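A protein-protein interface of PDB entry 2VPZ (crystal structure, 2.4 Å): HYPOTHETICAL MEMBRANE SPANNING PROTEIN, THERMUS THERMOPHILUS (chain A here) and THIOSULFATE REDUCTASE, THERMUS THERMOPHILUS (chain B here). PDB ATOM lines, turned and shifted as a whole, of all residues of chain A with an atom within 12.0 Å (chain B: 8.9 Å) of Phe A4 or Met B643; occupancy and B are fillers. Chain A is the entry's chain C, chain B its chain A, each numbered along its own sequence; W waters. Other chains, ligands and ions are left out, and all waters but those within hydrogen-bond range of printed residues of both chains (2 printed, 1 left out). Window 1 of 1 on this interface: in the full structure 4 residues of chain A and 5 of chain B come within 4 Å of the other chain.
The backbone carbonyl oxygen of Met B643 is in hydrogen-bond range of the backbone NH of Gly A6, 3.3 Å away.
The side-chain carboxylate of Glu A3 is in salt-bridge range of the guanidinium group of Arg B681 (3.4 Å).
Water W2 lies within hydrogen-bond range of the side-chain carboxylate of Glu A3 (2.5 Å) and the side-chain carboxylate of Glu B648 (3.0 Å).
Water W1 lies within hydrogen-bond range of the backbone carbonyl oxygen (O) of Phe A4 and the backbone carbonyl oxygen (O) of Met B643.
Of the 23 printed residues of chain B, 5 touch a printed residue of chain A.
Printed residues of chain B that touch a printed residue of chain A: Pro B627, Glu B642, Met B643, Asp B644 and Arg B681.
Hydrophobic or aromatic side chains of chain B that line the printed part of chain A: Pro B627 and Met B643.
Among the printed residues, 7 pairs touch across the chains.
OG of Ser B626 lies within hydrogen-bond range of OD2 of Asp B644.
The backbone carbonyl oxygen (O) of Asp B644 lies within hydrogen-bond range of a ring nitrogen (NE2) of His B629, 2.4 Å away.
The side-chain carboxylate (OD1) of Asp B644 lies close to the side-chain carboxylate (OE2) of Glu B648, 2.6 Å away.
The guanidinium group of Arg B681 lies within salt-bridge range of the side-chain carboxylate of Glu B646, 3.2 Å away.
Met B643 touches Phe A4.
Tyr A5 touches Pro B627.
Tyr A5 touches Met B643 (CD2 to O, 3.3 Å).
CE2 of Tyr A5 touches CB of Asp B644, at 3.99 Å.
CA of Gly A6 touches O of Glu B642, at 3.6 Å.
Of chain B, only Met B643 comes within 4 Å of Phe A4.
Of chain A, only Phe A4, Tyr A5 and Gly A6 come within 4 Å of Met B643.
Gly A6 touches just these residues of chain B: Glu B642 and Met B643.
No residue of chain A comes within 4 Å of Val B639.
No residue of chain A comes within 4 Å of Met B641.
Of the printed residues of chain A, Glu B642 touches Gly A6 (3.6 Å).
Of the printed residues of chain B, Glu A3 touches Arg B681.
Printed residues of chain A within 4 Å of Asp B644: Tyr A5 (3.99 Å).
Leu A251 touches none of the printed residues of chain B.
The nearest residue of chain B that does not touch Phe A4 is Asp B644 (5.7 Å).
The nearest residue of chain A that does not touch Met B643 is Leu A7 (6.2 Å).
The nearest printed residue of chain A that does not touch Asp B644 is Gly A6 (5.1 Å).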
ATOM      1  N   ALA A   2     -22.192 -26.558  -0.578  1.00  0.00           N
ATOM      2  CA  ALA A   2     -22.053 -27.181   0.768  1.00  0.00           C
ATOM      3  C   ALA A   2     -20.553 -27.126   1.205  1.00  0.00           C
ATOM      4  O   ALA A   2     -20.270 -26.657   2.309  1.00  0.00           O
ATOM      5  CB  ALA A   2     -22.623 -28.623   0.733  1.00  0.00           C
ATOM      6  N   GLU A   3     -19.614 -27.565   0.347  1.00  0.00           N
ATOM      7  CA  GLU A   3     -18.125 -27.515   0.576  1.00  0.00           C
ATOM      8  C   GLU A   3     -17.448 -26.428  -0.307  1.00  0.00           C
ATOM      9  O   GLU A   3     -17.866 -26.249  -1.452  1.00  0.00           O
ATOM     10  CB  GLU A   3     -17.417 -28.818   0.187  1.00  0.00           C
ATOM     11  CG  GLU A   3     -18.001 -30.069   0.750  1.00  0.00           C
ATOM     12  CD  GLU A   3     -17.709 -30.229   2.220  1.00  0.00           C
ATOM     13  OE1 GLU A   3     -16.576 -30.636   2.544  1.00  0.00           O
ATOM     14  OE2 GLU A   3     -18.605 -29.932   3.039  1.00  0.00           O
ATOM     15  N   PHE A   4     -16.406 -25.747   0.180  1.00  0.00           N
ATOM     16  CA  PHE A   4     -15.687 -24.724  -0.615  1.00  0.00           C
ATOM     17  C   PHE A   4     -14.154 -24.887  -0.656  1.00  0.00           C
ATOM     18  O   PHE A   4     -13.591 -25.618   0.149  1.00  0.00           O
ATOM     19  CB  PHE A   4     -15.881 -23.281  -0.066  1.00  0.00           C
ATOM     20  CG  PHE A   4     -17.307 -22.833   0.098  1.00  0.00           C
ATOM     21  CD1 PHE A   4     -17.996 -23.084   1.281  1.00  0.00           C
ATOM     22  CD2 PHE A   4     -17.962 -22.176  -0.943  1.00  0.00           C
ATOM     23  CE1 PHE A   4     -19.338 -22.688   1.435  1.00  0.00           C
ATOM     24  CE2 PHE A   4     -19.299 -21.769  -0.816  1.00  0.00           C
ATOM     25  CZ  PHE A   4     -19.993 -22.031   0.374  1.00  0.00           C
ATOM     26  N   TYR A   5     -13.515 -24.215  -1.628  1.00  0.00           N
ATOM     27  CA  TYR A   5     -12.050 -24.063  -1.690  1.00  0.00           C
ATOM     28  C   TYR A   5     -11.993 -22.537  -1.661  1.00  0.00           C
ATOM     29  O   TYR A   5     -12.464 -21.827  -2.579  1.00  0.00           O
ATOM     30  CB  TYR A   5     -11.355 -24.670  -2.897  1.00  0.00           C
ATOM     31  CG  TYR A   5     -11.249 -26.167  -2.755  1.00  0.00           C
ATOM     32  CD1 TYR A   5     -11.874 -26.998  -3.679  1.00  0.00           C
ATOM     33  CD2 TYR A   5     -10.582 -26.757  -1.677  1.00  0.00           C
ATOM     34  CE1 TYR A   5     -11.852 -28.373  -3.548  1.00  0.00           C
ATOM     35  CE2 TYR A   5     -10.543 -28.154  -1.524  1.00  0.00           C
ATOM     36  CZ  TYR A   5     -11.188 -28.960  -2.475  1.00  0.00           C
ATOM     37  OH  TYR A   5     -11.177 -30.335  -2.375  1.00  0.00           O
ATOM     38  N   GLY A   6     -11.455 -22.064  -0.543  1.00  0.00           N
ATOM     39  CA  GLY A   6     -11.462 -20.661  -0.249  1.00  0.00           C
ATOM     40  C   GLY A   6     -12.862 -20.522   0.364  1.00  0.00           C
ATOM     41  O   GLY A   6     -13.444 -21.519   0.821  1.00  0.00           O
ATOM     42  N   LEU A   7     -13.414 -19.310   0.321  1.00  0.00           N
ATOM     43  CA  LEU A   7     -14.734 -18.942   0.872  1.00  0.00           C
ATOM     44  C   LEU A   7     -15.380 -17.718   0.186  1.00  0.00           C
ATOM     45  O   LEU A   7     -14.647 -16.867  -0.325  1.00  0.00           O
ATOM     46  CB  LEU A   7     -14.606 -18.526   2.343  1.00  0.00           C
ATOM     47  CG  LEU A   7     -14.278 -19.512   3.458  1.00  0.00           C
ATOM     48  CD1 LEU A   7     -13.821 -18.758   4.741  1.00  0.00           C
ATOM     49  CD2 LEU A   7     -15.522 -20.407   3.685  1.00  0.00           C
ATOM     50  N   PRO A   8     -16.744 -17.643   0.123  1.00  0.00           N
ATOM     51  CA  PRO A   8     -17.395 -16.465  -0.482  1.00  0.00           C
ATOM     52  C   PRO A   8     -17.252 -15.385   0.602  1.00  0.00           C
ATOM     53  O   PRO A   8     -17.126 -15.736   1.781  1.00  0.00           O
ATOM     54  CB  PRO A   8     -18.877 -16.844  -0.617  1.00  0.00           C
ATOM     55  CG  PRO A   8     -19.054 -18.116   0.135  1.00  0.00           C
ATOM     56  CD  PRO A   8     -17.677 -18.775   0.188  1.00  0.00           C
ATOM     57  N   ASN A   9     -17.280 -14.110   0.220  1.00  0.00           N
ATOM     58  CA  ASN A   9     -17.178 -12.980   1.148  1.00  0.00           C
ATOM     59  C   ASN A   9     -18.579 -12.646   1.707  1.00  0.00           C
ATOM     60  O   ASN A   9     -19.168 -11.619   1.364  1.00  0.00           O
ATOM     61  CB  ASN A   9     -16.586 -11.773   0.416  1.00  0.00           C
ATOM     62  CG  ASN A   9     -15.241 -12.078  -0.233  1.00  0.00           C
ATOM     63  OD1 ASN A   9     -15.113 -12.090  -1.459  1.00  0.00           O
ATOM     64  ND2 ASN A   9     -14.241 -12.341   0.591  1.00  0.00           N
ATOM     65  N   ALA A  10     -19.113 -13.524   2.562  1.00  0.00           N
ATOM     66  CA  ALA A  10     -20.445 -13.393   3.139  1.00  0.00           C
ATOM     67  C   ALA A  10     -20.508 -12.993   4.614  1.00  0.00           C
ATOM     68  O   ALA A  10     -21.516 -13.237   5.284  1.00  0.00           O
ATOM     69  CB  ALA A  10     -21.241 -14.711   2.936  1.00  0.00           C
ATOM     70  N   GLN A  11     -19.440 -12.382   5.109  1.00  0.00           N
ATOM     71  CA  GLN A  11     -19.344 -11.932   6.499  1.00  0.00           C
ATOM     72  C   GLN A  11     -19.952 -10.524   6.721  1.00  0.00           C
ATOM     73  O   GLN A  11     -20.087  -9.732   5.789  1.00  0.00           O
ATOM     74  CB  GLN A  11     -17.885 -11.944   6.993  1.00  0.00           C
ATOM     75  CG  GLN A  11     -16.933 -10.979   6.246  1.00  0.00           C
ATOM     76  CD  GLN A  11     -16.415 -11.529   4.898  1.00  0.00           C
ATOM     77  OE1 GLN A  11     -15.879 -10.782   4.060  1.00  0.00           O
ATOM     78  NE2 GLN A  11     -16.552 -12.849   4.703  1.00  0.00           N
ATOM     79  N   GLN A 249     -28.137 -12.957   2.541  1.00  0.00           N
ATOM     80  CA  GLN A 249     -28.541 -13.112   1.109  1.00  0.00           C
ATOM     81  C   GLN A 249     -29.528 -14.269   0.974  1.00  0.00           C
ATOM     82  O   GLN A 249     -30.404 -14.320   0.078  1.00  0.00           O
ATOM     83  CB  GLN A 249     -27.358 -13.519   0.282  1.00  0.00           C
ATOM     84  CG  GLN A 249     -26.092 -12.765   0.432  1.00  0.00           C
ATOM     85  CD  GLN A 249     -25.984 -11.761  -0.665  1.00  0.00           C
ATOM     86  OE1 GLN A 249     -24.900 -11.375  -1.101  1.00  0.00           O
ATOM     87  NE2 GLN A 249     -27.150 -11.338  -1.158  1.00  0.00           N
ATOM     88  N   GLY A 250     -29.148 -15.223   1.815  1.00  0.00           N
ATOM     89  CA  GLY A 250     -29.711 -16.533   1.981  1.00  0.00           C
ATOM     90  C   GLY A 250     -30.728 -17.244   1.166  1.00  0.00           C
ATOM     91  O   GLY A 250     -31.789 -16.668   0.874  1.00  0.00           O
ATOM     92  N   LEU A 251     -30.414 -18.460   0.719  1.00  0.00           N
ATOM     93  CA  LEU A 251     -31.397 -19.304   0.023  1.00  0.00           C
ATOM     94  C   LEU A 251     -31.885 -20.441   1.043  1.00  0.00           C
ATOM     95  O   LEU A 251     -31.773 -20.322   2.312  1.00  0.00           O
ATOM     96  CB  LEU A 251     -30.910 -19.926  -1.343  1.00  0.00           C
ATOM     97  CG  LEU A 251     -30.182 -19.082  -2.450  1.00  0.00           C
ATOM     98  CD1 LEU A 251     -30.003 -19.797  -3.826  1.00  0.00           C
ATOM     99  CD2 LEU A 251     -30.943 -17.810  -2.712  1.00  0.00           C
ATOM    100  N   PRO B  80      -3.156 -26.145  -9.004  1.00  0.00           N
ATOM    101  CA  PRO B  80      -3.120 -25.285  -7.803  1.00  0.00           C
ATOM    102  C   PRO B  80      -1.808 -25.356  -6.972  1.00  0.00           C
ATOM    103  O   PRO B  80      -1.267 -24.332  -6.522  1.00  0.00           O
ATOM    104  CB  PRO B  80      -4.367 -25.702  -7.009  1.00  0.00           C
ATOM    105  CG  PRO B  80      -4.654 -27.133  -7.499  1.00  0.00           C
ATOM    106  CD  PRO B  80      -4.249 -27.123  -8.945  1.00  0.00           C
ATOM    107  N   ARG B  81      -1.296 -26.568  -6.763  1.00  0.00           N
ATOM    108  CA  ARG B  81      -0.058 -26.800  -6.009  1.00  0.00           C
ATOM    109  C   ARG B  81       1.156 -26.137  -6.668  1.00  0.00           C
ATOM    110  O   ARG B  81       2.061 -25.656  -5.969  1.00  0.00           O
ATOM    111  CB  ARG B  81       0.165 -28.315  -5.813  1.00  0.00           C
ATOM    112  CG  ARG B  81      -0.899 -28.925  -4.891  1.00  0.00           C
ATOM    113  CD  ARG B  81      -0.978 -30.459  -4.959  1.00  0.00           C
ATOM    114  NE  ARG B  81      -1.096 -31.003  -6.314  1.00  0.00           N
ATOM    115  CZ  ARG B  81      -0.193 -31.758  -6.939  1.00  0.00           C
ATOM    116  NH1 ARG B  81       0.935 -32.090  -6.339  1.00  0.00           N
ATOM    117  NH2 ARG B  81      -0.422 -32.159  -8.189  1.00  0.00           N
ATOM    118  N   GLN B  83       1.001 -23.401  -8.565  1.00  0.00           N
ATOM    119  CA  GLN B  83       0.782 -21.958  -8.380  1.00  0.00           C
ATOM    120  C   GLN B  83       1.135 -21.445  -6.968  1.00  0.00           C
ATOM    121  O   GLN B  83       1.699 -20.359  -6.830  1.00  0.00           O
ATOM    122  CB  GLN B  83      -0.666 -21.547  -8.720  1.00  0.00           C
ATOM    123  CG  GLN B  83      -1.130 -21.716 -10.192  1.00  0.00           C
ATOM    124  CD  GLN B  83      -0.618 -20.624 -11.149  1.00  0.00           C
ATOM    125  OE1 GLN B  83      -0.861 -20.673 -12.359  1.00  0.00           O
ATOM    126  NE2 GLN B  83       0.094 -19.627 -10.601  1.00  0.00           N
ATOM    127  N   GLY B  84       0.812 -22.215  -5.932  1.00  0.00           N
ATOM    128  CA  GLY B  84       1.124 -21.814  -4.574  1.00  0.00           C
ATOM    129  C   GLY B  84       2.467 -22.253  -4.021  1.00  0.00           C
ATOM    130  O   GLY B  84       2.947 -21.730  -3.013  1.00  0.00           O
ATOM    131  N   SER B 626      -6.063 -34.308  -1.727  1.00  0.00           N
ATOM    132  CA  SER B 626      -6.839 -33.037  -1.731  1.00  0.00           C
ATOM    133  C   SER B 626      -6.250 -32.317  -3.005  1.00  0.00           C
ATOM    134  O   SER B 626      -5.037 -32.180  -3.129  1.00  0.00           O
ATOM    135  CB  SER B 626      -6.579 -32.248  -0.424  1.00  0.00           C
ATOM    136  OG  SER B 626      -7.018 -30.914  -0.526  1.00  0.00           O
ATOM    137  N   PRO B 627      -7.125 -31.823  -3.932  1.00  0.00           N
ATOM    138  CA  PRO B 627      -6.569 -31.164  -5.135  1.00  0.00           C
ATOM    139  C   PRO B 627      -5.520 -30.043  -5.020  1.00  0.00           C
ATOM    140  O   PRO B 627      -4.766 -29.719  -5.969  1.00  0.00           O
ATOM    141  CB  PRO B 627      -7.811 -30.704  -5.919  1.00  0.00           C
ATOM    142  CG  PRO B 627      -8.847 -30.396  -4.802  1.00  0.00           C
ATOM    143  CD  PRO B 627      -8.547 -31.477  -3.738  1.00  0.00           C
ATOM    144  N   VAL B 628      -5.466 -29.516  -3.803  1.00  0.00           N
ATOM    145  CA  VAL B 628      -4.696 -28.346  -3.371  1.00  0.00           C
ATOM    146  C   VAL B 628      -3.485 -28.537  -2.408  1.00  0.00           C
ATOM    147  O   VAL B 628      -2.698 -27.613  -2.161  1.00  0.00           O
ATOM    148  CB  VAL B 628      -5.795 -27.388  -2.738  1.00  0.00           C
ATOM    149  CG1 VAL B 628      -5.208 -26.380  -1.801  1.00  0.00           C
ATOM    150  CG2 VAL B 628      -6.628 -26.701  -3.866  1.00  0.00           C
ATOM    151  N   HIS B 629      -3.335 -29.742  -1.856  1.00  0.00           N
ATOM    152  CA  HIS B 629      -2.253 -30.041  -0.941  1.00  0.00           C
ATOM    153  C   HIS B 629      -1.389 -31.202  -1.470  1.00  0.00           C
ATOM    154  O   HIS B 629      -1.908 -32.157  -2.062  1.00  0.00           O
ATOM    155  CB  HIS B 629      -2.827 -30.405   0.499  1.00  0.00           C
ATOM    156  CG  HIS B 629      -3.322 -29.255   1.325  1.00  0.00           C
ATOM    157  ND1 HIS B 629      -2.500 -28.321   1.884  1.00  0.00           N
ATOM    158  CD2 HIS B 629      -4.562 -28.902   1.678  1.00  0.00           C
ATOM    159  CE1 HIS B 629      -3.212 -27.429   2.536  1.00  0.00           C
ATOM    160  NE2 HIS B 629      -4.476 -27.762   2.424  1.00  0.00           N
ATOM    161  N   THR B 634       2.598 -29.248   2.621  1.00  0.00           N
ATOM    162  CA  THR B 634       1.937 -28.034   2.123  1.00  0.00           C
ATOM    163  C   THR B 634       0.947 -27.436   3.132  1.00  0.00           C
ATOM    164  O   THR B 634       0.288 -26.421   2.916  1.00  0.00           O
ATOM    165  CB  THR B 634       1.265 -28.435   0.771  1.00  0.00           C
ATOM    166  OG1 THR B 634       0.994 -27.283  -0.008  1.00  0.00           O
ATOM    167  CG2 THR B 634      -0.014 -29.217   1.042  1.00  0.00           C
ATOM    168  N   ASN B 637       1.669 -23.921   4.353  1.00  0.00           N
ATOM    169  CA  ASN B 637       1.560 -22.951   3.274  1.00  0.00           C
ATOM    170  C   ASN B 637       0.241 -22.125   3.444  1.00  0.00           C
ATOM    171  O   ASN B 637      -0.878 -22.640   3.308  1.00  0.00           O
ATOM    172  CB  ASN B 637       1.621 -23.704   1.937  1.00  0.00           C
ATOM    173  CG  ASN B 637       1.709 -22.780   0.754  1.00  0.00           C
ATOM    174  OD1 ASN B 637       0.977 -21.802   0.685  1.00  0.00           O
ATOM    175  ND2 ASN B 637       2.583 -23.084  -0.191  1.00  0.00           N
ATOM    176  N   TRP B 638       0.346 -20.832   3.749  1.00  0.00           N
ATOM    177  CA  TRP B 638      -0.864 -20.041   3.957  1.00  0.00           C
ATOM    178  C   TRP B 638      -1.776 -19.866   2.730  1.00  0.00           C
ATOM    179  O   TRP B 638      -2.995 -19.826   2.882  1.00  0.00           O
ATOM    180  CB  TRP B 638      -0.593 -18.673   4.647  1.00  0.00           C
ATOM    181  CG  TRP B 638      -0.058 -17.544   3.792  1.00  0.00           C
ATOM    182  CD1 TRP B 638       1.200 -17.023   3.823  1.00  0.00           C
ATOM    183  CD2 TRP B 638      -0.794 -16.720   2.839  1.00  0.00           C
ATOM    184  NE1 TRP B 638       1.302 -15.961   2.966  1.00  0.00           N
ATOM    185  CE2 TRP B 638       0.105 -15.751   2.344  1.00  0.00           C
ATOM    186  CE3 TRP B 638      -2.123 -16.718   2.349  1.00  0.00           C
ATOM    187  CZ2 TRP B 638      -0.264 -14.772   1.388  1.00  0.00           C
ATOM    188  CZ3 TRP B 638      -2.504 -15.729   1.380  1.00  0.00           C
ATOM    189  CH2 TRP B 638      -1.560 -14.783   0.914  1.00  0.00           C
ATOM    190  N   VAL B 639      -1.216 -19.804   1.524  1.00  0.00           N
ATOM    191  CA  VAL B 639      -2.040 -19.672   0.306  1.00  0.00           C
ATOM    192  C   VAL B 639      -2.880 -20.963   0.063  1.00  0.00           C
ATOM    193  O   VAL B 639      -4.018 -20.916  -0.399  1.00  0.00           O
ATOM    194  CB  VAL B 639      -1.152 -19.431  -0.978  1.00  0.00           C
ATOM    195  CG1 VAL B 639      -2.002 -19.520  -2.276  1.00  0.00           C
ATOM    196  CG2 VAL B 639      -0.445 -18.082  -0.875  1.00  0.00           C
ATOM    197  N   LEU B 640      -2.308 -22.107   0.413  1.00  0.00           N
ATOM    198  CA  LEU B 640      -2.943 -23.389   0.214  1.00  0.00           C
ATOM    199  C   LEU B 640      -3.794 -23.863   1.407  1.00  0.00           C
ATOM    200  O   LEU B 640      -4.832 -24.529   1.222  1.00  0.00           O
ATOM    201  CB  LEU B 640      -1.892 -24.443  -0.226  1.00  0.00           C
ATOM    202  CG  LEU B 640      -1.230 -24.212  -1.618  1.00  0.00           C
ATOM    203  CD1 LEU B 640      -0.089 -25.220  -1.860  1.00  0.00           C
ATOM    204  CD2 LEU B 640      -2.300 -24.288  -2.736  1.00  0.00           C
ATOM    205  N   MET B 641      -3.385 -23.519   2.622  1.00  0.00           N
ATOM    206  CA  MET B 641      -4.175 -23.885   3.805  1.00  0.00           C
ATOM    207  C   MET B 641      -5.506 -23.056   3.826  1.00  0.00           C
ATOM    208  O   MET B 641      -6.533 -23.491   4.337  1.00  0.00           O
ATOM    209  CB  MET B 641      -3.363 -23.675   5.097  1.00  0.00           C
ATOM    210  CG  MET B 641      -2.506 -24.883   5.524  1.00  0.00           C
ATOM    211  SD  MET B 641      -3.532 -26.367   5.856  1.00  0.00           S
ATOM    212  CE  MET B 641      -4.214 -25.927   7.522  1.00  0.00           C
ATOM    213  N   GLU B 642      -5.451 -21.868   3.231  1.00  0.00           N
ATOM    214  CA  GLU B 642      -6.594 -20.950   3.167  1.00  0.00           C
ATOM    215  C   GLU B 642      -7.665 -21.440   2.173  1.00  0.00           C
ATOM    216  O   GLU B 642      -8.829 -21.002   2.213  1.00  0.00           O
ATOM    217  CB  GLU B 642      -6.092 -19.562   2.812  1.00  0.00           C
ATOM    218  CG  GLU B 642      -7.032 -18.439   2.975  1.00  0.00           C
ATOM    219  CD  GLU B 642      -6.305 -17.127   2.780  1.00  0.00           C
ATOM    220  OE1 GLU B 642      -5.818 -16.903   1.644  1.00  0.00           O
ATOM    221  OE2 GLU B 642      -6.172 -16.368   3.765  1.00  0.00           O
ATOM    222  N   MET B 643      -7.253 -22.338   1.273  1.00  0.00           N
ATOM    223  CA  MET B 643      -8.165 -22.987   0.325  1.00  0.00           C
ATOM    224  C   MET B 643      -8.703 -24.286   0.996  1.00  0.00           C
ATOM    225  O   MET B 643      -9.819 -24.689   0.731  1.00  0.00           O
ATOM    226  CB  MET B 643      -7.486 -23.394  -0.992  1.00  0.00           C
ATOM    227  CG  MET B 643      -6.916 -22.244  -1.800  1.00  0.00           C
ATOM    228  SD  MET B 643      -8.232 -21.215  -2.531  1.00  0.00           S
ATOM    229  CE  MET B 643      -7.251 -19.833  -3.236  1.00  0.00           C
ATOM    230  N   ASP B 644      -7.907 -24.919   1.861  1.00  0.00           N
ATOM    231  CA  ASP B 644      -8.274 -26.208   2.517  1.00  0.00           C
ATOM    232  C   ASP B 644      -7.461 -26.358   3.801  1.00  0.00           C
ATOM    233  O   ASP B 644      -6.342 -26.984   3.803  1.00  0.00           O
ATOM    234  CB  ASP B 644      -8.058 -27.358   1.499  1.00  0.00           C
ATOM    235  CG  ASP B 644      -8.633 -28.697   1.973  1.00  0.00           C
ATOM    236  OD1 ASP B 644      -9.603 -28.687   2.787  1.00  0.00           O
ATOM    237  OD2 ASP B 644      -8.125 -29.754   1.495  1.00  0.00           O
ATOM    238  N   PRO B 645      -8.005 -25.828   4.941  1.00  0.00           N
ATOM    239  CA  PRO B 645      -7.503 -25.775   6.310  1.00  0.00           C
ATOM    240  C   PRO B 645      -7.634 -27.031   7.158  1.00  0.00           C
ATOM    241  O   PRO B 645      -7.088 -27.099   8.265  1.00  0.00           O
ATOM    242  CB  PRO B 645      -8.250 -24.565   6.901  1.00  0.00           C
ATOM    243  CG  PRO B 645      -9.525 -24.404   6.005  1.00  0.00           C
ATOM    244  CD  PRO B 645      -9.434 -25.577   4.992  1.00  0.00           C
ATOM    245  N   GLU B 646      -8.392 -28.003   6.679  1.00  0.00           N
ATOM    246  CA  GLU B 646      -8.570 -29.255   7.421  1.00  0.00           C
ATOM    247  C   GLU B 646      -9.171 -30.363   6.558  1.00  0.00           C
ATOM    248  O   GLU B 646      -9.738 -30.083   5.479  1.00  0.00           O
ATOM    249  CB  GLU B 646      -9.474 -29.064   8.658  1.00  0.00           C
ATOM    250  CG  GLU B 646     -10.826 -28.329   8.332  1.00  0.00           C
ATOM    251  CD  GLU B 646     -11.943 -28.443   9.408  1.00  0.00           C
ATOM    252  OE1 GLU B 646     -11.700 -29.070  10.457  1.00  0.00           O
ATOM    253  OE2 GLU B 646     -13.063 -27.912   9.188  1.00  0.00           O
ATOM    254  N   GLU B 648     -11.685 -33.833   6.347  1.00  0.00           N
ATOM    255  CA  GLU B 648     -13.067 -34.057   6.690  1.00  0.00           C
ATOM    256  C   GLU B 648     -13.322 -35.646   6.497  1.00  0.00           C
ATOM    257  O   GLU B 648     -12.901 -36.220   5.491  1.00  0.00           O
ATOM    258  CB  GLU B 648     -13.736 -33.022   5.666  1.00  0.00           C
ATOM    259  CG  GLU B 648     -12.909 -31.533   5.506  1.00  0.00           C
ATOM    260  CD  GLU B 648     -12.193 -31.214   4.114  1.00  0.00           C
ATOM    261  OE1 GLU B 648     -12.429 -31.955   3.136  1.00  0.00           O
ATOM    262  OE2 GLU B 648     -11.394 -30.196   3.987  1.00  0.00           O
ATOM    263  N   ARG B 681     -13.512 -33.099  11.254  1.00  0.00           N
ATOM    264  CA  ARG B 681     -14.885 -32.782  10.932  1.00  0.00           C
ATOM    265  C   ARG B 681     -15.576 -33.967  10.241  1.00  0.00           C
ATOM    266  O   ARG B 681     -14.959 -34.684   9.433  1.00  0.00           O
ATOM    267  CB  ARG B 681     -14.994 -31.519  10.069  1.00  0.00           C
ATOM    268  CG  ARG B 681     -16.115 -30.598  10.510  1.00  0.00           C
ATOM    269  CD  ARG B 681     -16.283 -29.403   9.557  1.00  0.00           C
ATOM    270  NE  ARG B 681     -16.828 -29.777   8.256  1.00  0.00           N
ATOM    271  CZ  ARG B 681     -16.189 -29.712   7.080  1.00  0.00           C
ATOM    272  NH1 ARG B 681     -14.942 -29.279   7.009  1.00  0.00           N
ATOM    273  NH2 ARG B 681     -16.823 -30.071   5.950  1.00  0.00           N
ATOM    274  N   PHE B 699      -2.621 -34.661   7.039  1.00  0.00           N
ATOM    275  CA  PHE B 699      -3.001 -33.698   8.092  1.00  0.00           C
ATOM    276  C   PHE B 699      -2.648 -34.337   9.453  1.00  0.00           C
ATOM    277  O   PHE B 699      -2.031 -35.413   9.477  1.00  0.00           O
ATOM    278  CB  PHE B 699      -4.490 -33.305   8.036  1.00  0.00           C
ATOM    279  CG  PHE B 699      -4.838 -32.311   6.928  1.00  0.00           C
ATOM    280  CD1 PHE B 699      -5.089 -32.757   5.630  1.00  0.00           C
ATOM    281  CD2 PHE B 699      -4.908 -30.934   7.190  1.00  0.00           C
ATOM    282  CE1 PHE B 699      -5.403 -31.848   4.600  1.00  0.00           C
ATOM    283  CE2 PHE B 699      -5.221 -30.006   6.193  1.00  0.00           C
ATOM    284  CZ  PHE B 699      -5.469 -30.463   4.885  1.00  0.00           C
ATOM    285  N   LEU B 752      -6.056 -18.675  11.465  1.00  0.00           N
ATOM    286  CA  LEU B 752      -5.180 -18.873  10.303  1.00  0.00           C
ATOM    287  C   LEU B 752      -4.807 -17.576   9.579  1.00  0.00           C
ATOM    288  O   LEU B 752      -3.687 -17.459   9.072  1.00  0.00           O
ATOM    289  CB  LEU B 752      -5.797 -19.813   9.267  1.00  0.00           C
ATOM    290  CG  LEU B 752      -5.371 -21.270   9.263  1.00  0.00           C
ATOM    291  CD1 LEU B 752      -6.147 -21.998   8.165  1.00  0.00           C
ATOM    292  CD2 LEU B 752      -3.858 -21.389   9.033  1.00  0.00           C
HETATM  293  O   HOH W   1     -12.014 -25.705   2.180  1.00  0.00           O
HETATM  294  O   HOH W   2     -14.975 -32.417   1.680  1.00  0.00           O
